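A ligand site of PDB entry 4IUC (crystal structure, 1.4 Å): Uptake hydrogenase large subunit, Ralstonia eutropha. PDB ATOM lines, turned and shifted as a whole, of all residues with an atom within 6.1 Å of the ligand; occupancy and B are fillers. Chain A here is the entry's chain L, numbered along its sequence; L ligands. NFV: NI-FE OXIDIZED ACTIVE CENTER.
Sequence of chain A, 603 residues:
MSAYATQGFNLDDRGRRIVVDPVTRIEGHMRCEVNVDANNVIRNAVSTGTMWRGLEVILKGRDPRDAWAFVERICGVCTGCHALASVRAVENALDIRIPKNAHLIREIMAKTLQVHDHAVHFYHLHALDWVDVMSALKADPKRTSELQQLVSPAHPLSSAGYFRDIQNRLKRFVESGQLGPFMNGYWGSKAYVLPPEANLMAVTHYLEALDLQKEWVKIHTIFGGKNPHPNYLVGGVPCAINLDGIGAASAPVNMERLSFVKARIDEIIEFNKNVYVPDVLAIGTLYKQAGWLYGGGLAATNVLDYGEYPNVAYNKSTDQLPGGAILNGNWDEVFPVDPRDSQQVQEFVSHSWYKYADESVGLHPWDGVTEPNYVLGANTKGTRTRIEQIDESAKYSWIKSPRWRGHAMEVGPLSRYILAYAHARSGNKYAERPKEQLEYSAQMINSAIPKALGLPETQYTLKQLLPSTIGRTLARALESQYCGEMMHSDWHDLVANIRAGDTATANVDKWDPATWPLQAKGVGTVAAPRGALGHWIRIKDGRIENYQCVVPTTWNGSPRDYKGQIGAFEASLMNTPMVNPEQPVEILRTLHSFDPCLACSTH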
ATOM      1  N   GLU A  27      13.375 -18.861  25.567  1.00  0.00           N
ATOM      2  CA  GLU A  27      12.358 -18.681  24.552  1.00  0.00           C
ATOM      3  C   GLU A  27      11.479 -17.511  24.961  1.00  0.00           C
ATOM      4  O   GLU A  27      11.025 -17.426  26.113  1.00  0.00           O
ATOM      5  CB  GLU A  27      11.512 -19.961  24.367  1.00  0.00           C
ATOM      6  CG  GLU A  27      10.560 -19.937  23.164  1.00  0.00           C
ATOM      7  CD  GLU A  27       9.425 -18.923  23.306  1.00  0.00           C
ATOM      8  OE1 GLU A  27       8.979 -18.678  24.444  1.00  0.00           O
ATOM      9  OE2 GLU A  27       8.974 -18.346  22.276  1.00  0.00           O
ATOM     10  N   ILE A  74       1.585 -22.664  20.450  1.00  0.00           N
ATOM     11  CA  ILE A  74       1.997 -21.979  21.662  1.00  0.00           C
ATOM     12  C   ILE A  74       3.539 -21.917  21.696  1.00  0.00           C
ATOM     13  O   ILE A  74       4.114 -20.934  22.180  1.00  0.00           O
ATOM     14  CB  ILE A  74       1.440 -22.665  22.930  1.00  0.00           C
ATOM     15  CG1 ILE A  74      -0.071 -22.387  23.010  1.00  0.00           C
ATOM     16  CG2 ILE A  74       2.169 -22.187  24.180  1.00  0.00           C
ATOM     17  CD1 ILE A  74      -0.784 -23.192  24.086  1.00  0.00           C
ATOM     18  N   CYS A  75       4.199 -22.954  21.193  1.00  0.00           N
ATOM     19  CA  CYS A  75       5.648 -23.023  21.318  1.00  0.00           C
ATOM     20  C   CYS A  75       6.303 -23.950  20.332  1.00  0.00           C
ATOM     21  O   CYS A  75       5.918 -25.131  20.211  1.00  0.00           O
ATOM     22  CB  CYS A  75       6.014 -23.449  22.722  1.00  0.00           C
ATOM     23  SG  CYS A  75       7.772 -23.253  23.062  1.00  0.00           S
ATOM     24  N   GLY A  76       7.325 -23.430  19.666  1.00  0.00           N
ATOM     25  CA  GLY A  76       8.100 -24.194  18.689  1.00  0.00           C
ATOM     26  C   GLY A  76       9.356 -24.812  19.283  1.00  0.00           C
ATOM     27  O   GLY A  76      10.067 -25.548  18.592  1.00  0.00           O
ATOM     28  N   VAL A  77       9.630 -24.492  20.549  1.00  0.00           N
ATOM     29  CA  VAL A  77      10.766 -25.098  21.254  1.00  0.00           C
ATOM     30  C   VAL A  77      10.324 -26.407  21.878  1.00  0.00           C
ATOM     31  O   VAL A  77      10.850 -27.482  21.542  1.00  0.00           O
ATOM     32  CB  VAL A  77      11.367 -24.136  22.315  1.00  0.00           C
ATOM     33  CG1 VAL A  77      12.494 -24.825  23.083  1.00  0.00           C
ATOM     34  CG2 VAL A  77      11.885 -22.875  21.637  1.00  0.00           C
ATOM     35  N   CYS A  78       9.304 -26.344  22.732  1.00  0.00           N
ATOM     36  CA  CYS A  78       8.689 -27.572  23.243  1.00  0.00           C
ATOM     37  C   CYS A  78       7.655 -28.067  22.233  1.00  0.00           C
ATOM     38  O   CYS A  78       6.482 -28.314  22.556  1.00  0.00           O
ATOM     39  CB  CYS A  78       8.106 -27.366  24.655  1.00  0.00           C
ATOM     40  SG  CYS A  78       6.872 -26.044  24.848  1.00  0.00           S
ATOM     41  N   THR A  79       8.085 -28.201  20.986  1.00  0.00           N
ATOM     42  CA  THR A  79       7.154 -28.453  19.896  1.00  0.00           C
ATOM     43  C   THR A  79       6.485 -29.838  19.969  1.00  0.00           C
ATOM     44  O   THR A  79       7.157 -30.873  20.018  1.00  0.00           O
ATOM     45  CB  THR A  79       7.842 -28.227  18.537  1.00  0.00           C
ATOM     46  OG1 THR A  79       6.886 -28.431  17.499  1.00  0.00           O
ATOM     47  CG2 THR A  79       9.019 -29.189  18.334  1.00  0.00           C
ATOM     48  N   CYS A  81       4.408 -30.889  22.439  1.00  0.00           N
ATOM     49  CA  CYS A  81       3.883 -31.266  23.764  1.00  0.00           C
ATOM     50  C   CYS A  81       2.491 -30.712  23.966  1.00  0.00           C
ATOM     51  O   CYS A  81       1.649 -31.359  24.587  1.00  0.00           O
ATOM     52  CB  CYS A  81       4.822 -30.926  24.921  1.00  0.00           C
ATOM     53  SG  CYS A  81       4.935 -29.174  25.360  1.00  0.00           S
ATOM     54  N   HIS A  82       2.216 -29.523  23.415  1.00  0.00           N
ATOM     55  CA  HIS A  82       0.842 -28.981  23.495  1.00  0.00           C
ATOM     56  C   HIS A  82      -0.117 -29.732  22.632  1.00  0.00           C
ATOM     57  O   HIS A  82      -1.302 -29.858  22.970  1.00  0.00           O
ATOM     58  CB  HIS A  82       0.826 -27.510  23.129  1.00  0.00           C
ATOM     59  CG  HIS A  82       1.447 -26.634  24.165  1.00  0.00           C
ATOM     60  ND1 HIS A  82       0.859 -26.373  25.366  1.00  0.00           N
ATOM     61  CD2 HIS A  82       2.663 -25.958  24.172  1.00  0.00           C
ATOM     62  CE1 HIS A  82       1.659 -25.569  26.086  1.00  0.00           C
ATOM     63  NE2 HIS A  82       2.748 -25.310  25.349  1.00  0.00           N
ATOM     64  N   ASP A 117      15.069 -30.991  23.355  1.00  0.00           N
ATOM     65  CA  ASP A 117      14.838 -29.768  24.097  1.00  0.00           C
ATOM     66  C   ASP A 117      15.888 -29.633  25.224  1.00  0.00           C
ATOM     67  O   ASP A 117      16.556 -28.588  25.350  1.00  0.00           O
ATOM     68  CB  ASP A 117      13.406 -29.804  24.660  1.00  0.00           C
ATOM     69  CG  ASP A 117      12.832 -28.441  24.901  1.00  0.00           C
ATOM     70  OD1 ASP A 117      13.606 -27.513  25.243  1.00  0.00           O
ATOM     71  OD2 ASP A 117      11.582 -28.307  24.801  1.00  0.00           O
ATOM     72  N   ALA A 528       5.822 -32.262  30.252  1.00  0.00           N
ATOM     73  CA  ALA A 528       6.543 -31.532  29.214  1.00  0.00           C
ATOM     74  C   ALA A 528       7.976 -31.278  29.684  1.00  0.00           C
ATOM     75  O   ALA A 528       8.273 -31.395  30.881  1.00  0.00           O
ATOM     76  CB  ALA A 528       5.811 -30.237  28.939  1.00  0.00           C
ATOM     77  N   PRO A 529       8.879 -30.929  28.748  1.00  0.00           N
ATOM     78  CA  PRO A 529      10.273 -30.726  29.125  1.00  0.00           C
ATOM     79  C   PRO A 529      10.490 -29.820  30.354  1.00  0.00           C
ATOM     80  O   PRO A 529      11.410 -30.073  31.125  1.00  0.00           O
ATOM     81  CB  PRO A 529      10.893 -30.122  27.873  1.00  0.00           C
ATOM     82  CG  PRO A 529      10.123 -30.789  26.774  1.00  0.00           C
ATOM     83  CD  PRO A 529       8.698 -30.881  27.294  1.00  0.00           C
ATOM     84  N   ARG A 530       9.635 -28.809  30.535  1.00  0.00           N
ATOM     85  CA  ARG A 530       9.829 -27.843  31.622  1.00  0.00           C
ATOM     86  C   ARG A 530       8.975 -28.107  32.865  1.00  0.00           C
ATOM     87  O   ARG A 530       9.068 -27.363  33.845  1.00  0.00           O
ATOM     88  CB  ARG A 530       9.635 -26.412  31.112  1.00  0.00           C
ATOM     89  CG  ARG A 530      10.744 -25.985  30.172  1.00  0.00           C
ATOM     90  CD  ARG A 530      10.281 -24.938  29.173  1.00  0.00           C
ATOM     91  NE  ARG A 530      11.365 -24.685  28.218  1.00  0.00           N
ATOM     92  CZ  ARG A 530      11.636 -25.452  27.159  1.00  0.00           C
ATOM     93  NH1 ARG A 530      10.822 -26.455  26.827  1.00  0.00           N
ATOM     94  NH2 ARG A 530      12.693 -25.178  26.406  1.00  0.00           N
ATOM     95  N   GLY A 531       8.156 -29.148  32.830  1.00  0.00           N
ATOM     96  CA  GLY A 531       7.368 -29.518  34.009  1.00  0.00           C
ATOM     97  C   GLY A 531       5.953 -29.899  33.652  1.00  0.00           C
ATOM     98  O   GLY A 531       5.704 -30.525  32.636  1.00  0.00           O
ATOM     99  N   LEU A 533       2.322 -29.866  32.471  1.00  0.00           N
ATOM    100  CA  LEU A 533       1.465 -29.216  31.480  1.00  0.00           C
ATOM    101  C   LEU A 533       0.064 -29.802  31.546  1.00  0.00           C
ATOM    102  O   LEU A 533      -0.103 -31.032  31.575  1.00  0.00           O
ATOM    103  CB  LEU A 533       2.032 -29.414  30.060  1.00  0.00           C
ATOM    104  CG  LEU A 533       1.122 -29.028  28.872  1.00  0.00           C
ATOM    105  CD1 LEU A 533       0.797 -27.539  28.917  1.00  0.00           C
ATOM    106  CD2 LEU A 533       1.772 -29.399  27.536  1.00  0.00           C
ATOM    107  N   VAL A 551       0.646 -24.061  31.982  1.00  0.00           N
ATOM    108  CA  VAL A 551       1.834 -24.540  31.299  1.00  0.00           C
ATOM    109  C   VAL A 551       3.014 -24.499  32.316  1.00  0.00           C
ATOM    110  O   VAL A 551       2.963 -23.752  33.298  1.00  0.00           O
ATOM    111  CB  VAL A 551       2.024 -23.663  30.030  1.00  0.00           C
ATOM    112  CG1 VAL A 551       3.179 -24.121  29.161  1.00  0.00           C
ATOM    113  CG2 VAL A 551       0.743 -23.640  29.186  1.00  0.00           C
ATOM    114  N   PRO A 552       4.050 -25.350  32.115  1.00  0.00           N
ATOM    115  CA  PRO A 552       5.083 -25.438  33.160  1.00  0.00           C
ATOM    116  C   PRO A 552       5.687 -24.077  33.551  1.00  0.00           C
ATOM    117  O   PRO A 552       5.837 -23.792  34.742  1.00  0.00           O
ATOM    118  CB  PRO A 552       6.130 -26.359  32.542  1.00  0.00           C
ATOM    119  CG  PRO A 552       5.328 -27.258  31.659  1.00  0.00           C
ATOM    120  CD  PRO A 552       4.230 -26.402  31.093  1.00  0.00           C
ATOM    121  N   THR A 553       6.052 -23.257  32.562  1.00  0.00           N
ATOM    122  CA  THR A 553       6.664 -21.975  32.861  1.00  0.00           C
ATOM    123  C   THR A 553       5.619 -20.983  33.445  1.00  0.00           C
ATOM    124  O   THR A 553       5.991 -19.999  34.101  1.00  0.00           O
ATOM    125  CB  THR A 553       7.415 -21.392  31.642  1.00  0.00           C
ATOM    126  OG1 THR A 553       8.391 -22.341  31.193  1.00  0.00           O
ATOM    127  CG2 THR A 553       8.159 -20.087  32.014  1.00  0.00           C
ATOM    128  N   THR A 554       4.330 -21.279  33.257  1.00  0.00           N
ATOM    129  CA  THR A 554       3.298 -20.516  33.991  1.00  0.00           C
ATOM    130  C   THR A 554       3.493 -20.727  35.508  1.00  0.00           C
ATOM    131  O   THR A 554       3.520 -19.776  36.274  1.00  0.00           O
ATOM    132  CB  THR A 554       1.849 -20.904  33.597  1.00  0.00           C
ATOM    133  OG1 THR A 554       1.740 -21.021  32.159  1.00  0.00           O
ATOM    134  CG2 THR A 554       0.878 -19.858  34.103  1.00  0.00           C
ATOM    135  N   ASP A 595      14.948 -23.260  32.464  1.00  0.00           N
ATOM    136  CA  ASP A 595      14.668 -23.362  31.046  1.00  0.00           C
ATOM    137  C   ASP A 595      13.345 -22.590  30.717  1.00  0.00           C
ATOM    138  O   ASP A 595      12.351 -23.159  30.252  1.00  0.00           O
ATOM    139  CB  ASP A 595      14.614 -24.857  30.707  1.00  0.00           C
ATOM    140  CG  ASP A 595      14.332 -25.152  29.280  1.00  0.00           C
ATOM    141  OD1 ASP A 595      14.467 -24.255  28.393  1.00  0.00           O
ATOM    142  OD2 ASP A 595      13.970 -26.332  29.037  1.00  0.00           O
ATOM    143  N   PRO A 596      13.322 -21.268  30.997  1.00  0.00           N
ATOM    144  CA  PRO A 596      12.095 -20.512  30.802  1.00  0.00           C
ATOM    145  C   PRO A 596      11.625 -20.519  29.346  1.00  0.00           C
ATOM    146  O   PRO A 596      12.412 -20.227  28.418  1.00  0.00           O
ATOM    147  CB  PRO A 596      12.482 -19.085  31.233  1.00  0.00           C
ATOM    148  CG  PRO A 596      13.672 -19.262  32.117  1.00  0.00           C
ATOM    149  CD  PRO A 596      14.406 -20.431  31.534  1.00  0.00           C
ATOM    150  N   CYS A 597      10.342 -20.795  29.165  1.00  0.00           N
ATOM    151  CA  CYS A 597       9.702 -20.669  27.865  1.00  0.00           C
ATOM    152  C   CYS A 597       8.533 -19.709  28.026  1.00  0.00           C
ATOM    153  O   CYS A 597       7.500 -20.051  28.613  1.00  0.00           O
ATOM    154  CB  CYS A 597       9.227 -22.007  27.354  1.00  0.00           C
ATOM    155  SG  CYS A 597       8.644 -21.893  25.647  1.00  0.00           S
ATOM    156  N   LEU A 598       8.746 -18.472  27.582  1.00  0.00           N
ATOM    157  CA  LEU A 598       7.828 -17.415  27.938  1.00  0.00           C
ATOM    158  C   LEU A 598       6.582 -17.438  27.054  1.00  0.00           C
ATOM    159  O   LEU A 598       5.495 -17.084  27.527  1.00  0.00           O
ATOM    160  CB  LEU A 598       8.540 -16.060  27.926  1.00  0.00           C
ATOM    161  CG  LEU A 598       9.276 -15.718  29.254  1.00  0.00           C
ATOM    162  CD1 LEU A 598       8.303 -15.327  30.355  1.00  0.00           C
ATOM    163  CD2 LEU A 598      10.195 -16.832  29.741  1.00  0.00           C
ATOM    164  N   ALA A 599       6.738 -17.859  25.794  1.00  0.00           N
ATOM    165  CA  ALA A 599       5.568 -18.072  24.940  1.00  0.00           C
ATOM    166  C   ALA A 599       4.672 -19.168  25.538  1.00  0.00           C
ATOM    167  O   ALA A 599       3.422 -19.022  25.575  1.00  0.00           O
ATOM    168  CB  ALA A 599       6.004 -18.444  23.524  1.00  0.00           C
ATOM    169  N   CYS A 600       5.288 -20.223  26.061  1.00  0.00           N
ATOM    170  CA  CYS A 600       4.518 -21.232  26.783  1.00  0.00           C
ATOM    171  C   CYS A 600       3.823 -20.650  27.990  1.00  0.00           C
ATOM    172  O   CYS A 600       2.650 -20.942  28.243  1.00  0.00           O
ATOM    173  CB  CYS A 600       5.443 -22.333  27.270  1.00  0.00           C
ATOM    174  SG  CYS A 600       5.453 -23.765  26.184  1.00  0.00           S
ATOM    175  N   SER A 601       4.535 -19.839  28.750  1.00  0.00           N
ATOM    176  CA  SER A 601       4.008 -19.391  30.055  1.00  0.00           C
ATOM    177  C   SER A 601       2.750 -18.545  29.911  1.00  0.00           C
ATOM    178  O   SER A 601       1.888 -18.547  30.801  1.00  0.00           O
ATOM    179  CB  SER A 601       5.072 -18.600  30.838  1.00  0.00           C
ATOM    180  OG  SER A 601       5.264 -17.296  30.305  1.00  0.00           O
HETATM  181 FE   NFV L   1       6.601 -25.571  27.149  1.00  0.00          FE
HETATM  182 NI   NFV L   1       7.893 -23.929  25.131  1.00  0.00          NI
HETATM  183  C1  NFV L   1       5.023 -26.476  27.547  1.00  0.00           C
HETATM  184  O1  NFV L   1       4.085 -27.029  27.782  1.00  0.00           O
HETATM  185  C2  NFV L   1       7.596 -27.037  27.860  1.00  0.00           C
HETATM  186  N2  NFV L   1       8.195 -27.903  28.278  1.00  0.00           N
HETATM  187  C3  NFV L   1       6.675 -24.734  28.909  1.00  0.00           C
HETATM  188  N3  NFV L   1       6.721 -24.241  29.917  1.00  0.00           N
HETATM  189  O4  NFV L   1       8.315 -24.643  26.764  1.00  0.00           O
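The side-chain carboxylate (OD1) of Asp 595 is in salt-bridge range of the guanidinium group (NH2) of Arg 530, at 2.8 Å.
N of Val 77 lies close to SG of Cys 75 (3.4 Å).
The backbone carbonyl oxygen (O) of Cys 78 is in hydrogen-bond range of the side-chain sulfur (SG) of Cys 81 (3.3 Å).
The side-chain sulfur of Cys 597 lies close to the side-chain carboxylate of Glu 27 (3.4 Å).
The backbone NH (N) of Cys 597 lies within hydrogen-bond range of the side-chain hydroxyl (OG1) of Thr 553, at 3.2 Å.
The guanidinium group (NH2) of Arg 530 lies within salt-bridge range of the side-chain carboxylate (OD1) of Asp 117, 2.8 Å away.
The backbone carbonyl oxygen (O) of Val 551 lies close to the side-chain hydroxyl (OG1) of Thr 554 (3.2 Å).
The side-chain sulfur (SG) of Cys 600 lies close to a ring nitrogen (NE2) of His 82 (3.2 Å).
The backbone NH of Arg 530 sits at hydrogen-bond distance from a nitrogen (N2) of the ligand (2.8 Å).
The guanidinium group (NH1) of Arg 530 is in hydrogen-bond range of a nitrogen (N2) of the ligand (3.3 Å).
A nickel atom (NI) of the ligand is bound by the side-chain sulfur (SG) of Cys 75, 2.2 Å away.
SG of Cys 600 is bound to FE of the ligand, at 2.3 Å.
N3 of the ligand sits at hydrogen-bond distance from N of Thr 553, at 2.9 Å.
An iron atom (FE) of the ligand is bound by the side-chain sulfur of Cys 78 (2.4 Å).
A nitrogen (N3) of the ligand is in hydrogen-bond range of the side-chain hydroxyl (OG1) of Thr 553 (2.8 Å).
An oxygen (O1) of the ligand is in hydrogen-bond range of the side-chain sulfur of Cys 81 (3.3 Å).
NI of the ligand is bound by SG of Cys 597 (2.2 Å).
A ring nitrogen (NE2) of His 82 sits at hydrogen-bond distance from an oxygen (O1) of the ligand (3.3 Å).
The backbone nitrogen of Pro 529 sits close to a nitrogen (N2) of the ligand, at 3.1 Å.
Merely in contact with the ligand: Leu 533, Val 551, Pro 552 and Ala 528.
Hydrophobic or aromatic side chains that line the ligand: His 82, Ala 528, Pro 529, Leu 533, Val 551 and Pro 552.
13 residues have an atom within 4 Å of the ligand: Cys 75, Cys 78, Cys 81, His 82, Ala 528, Pro 529, Arg 530, Leu 533, Val 551, Pro 552, Thr 553, Cys 597 and Cys 600.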
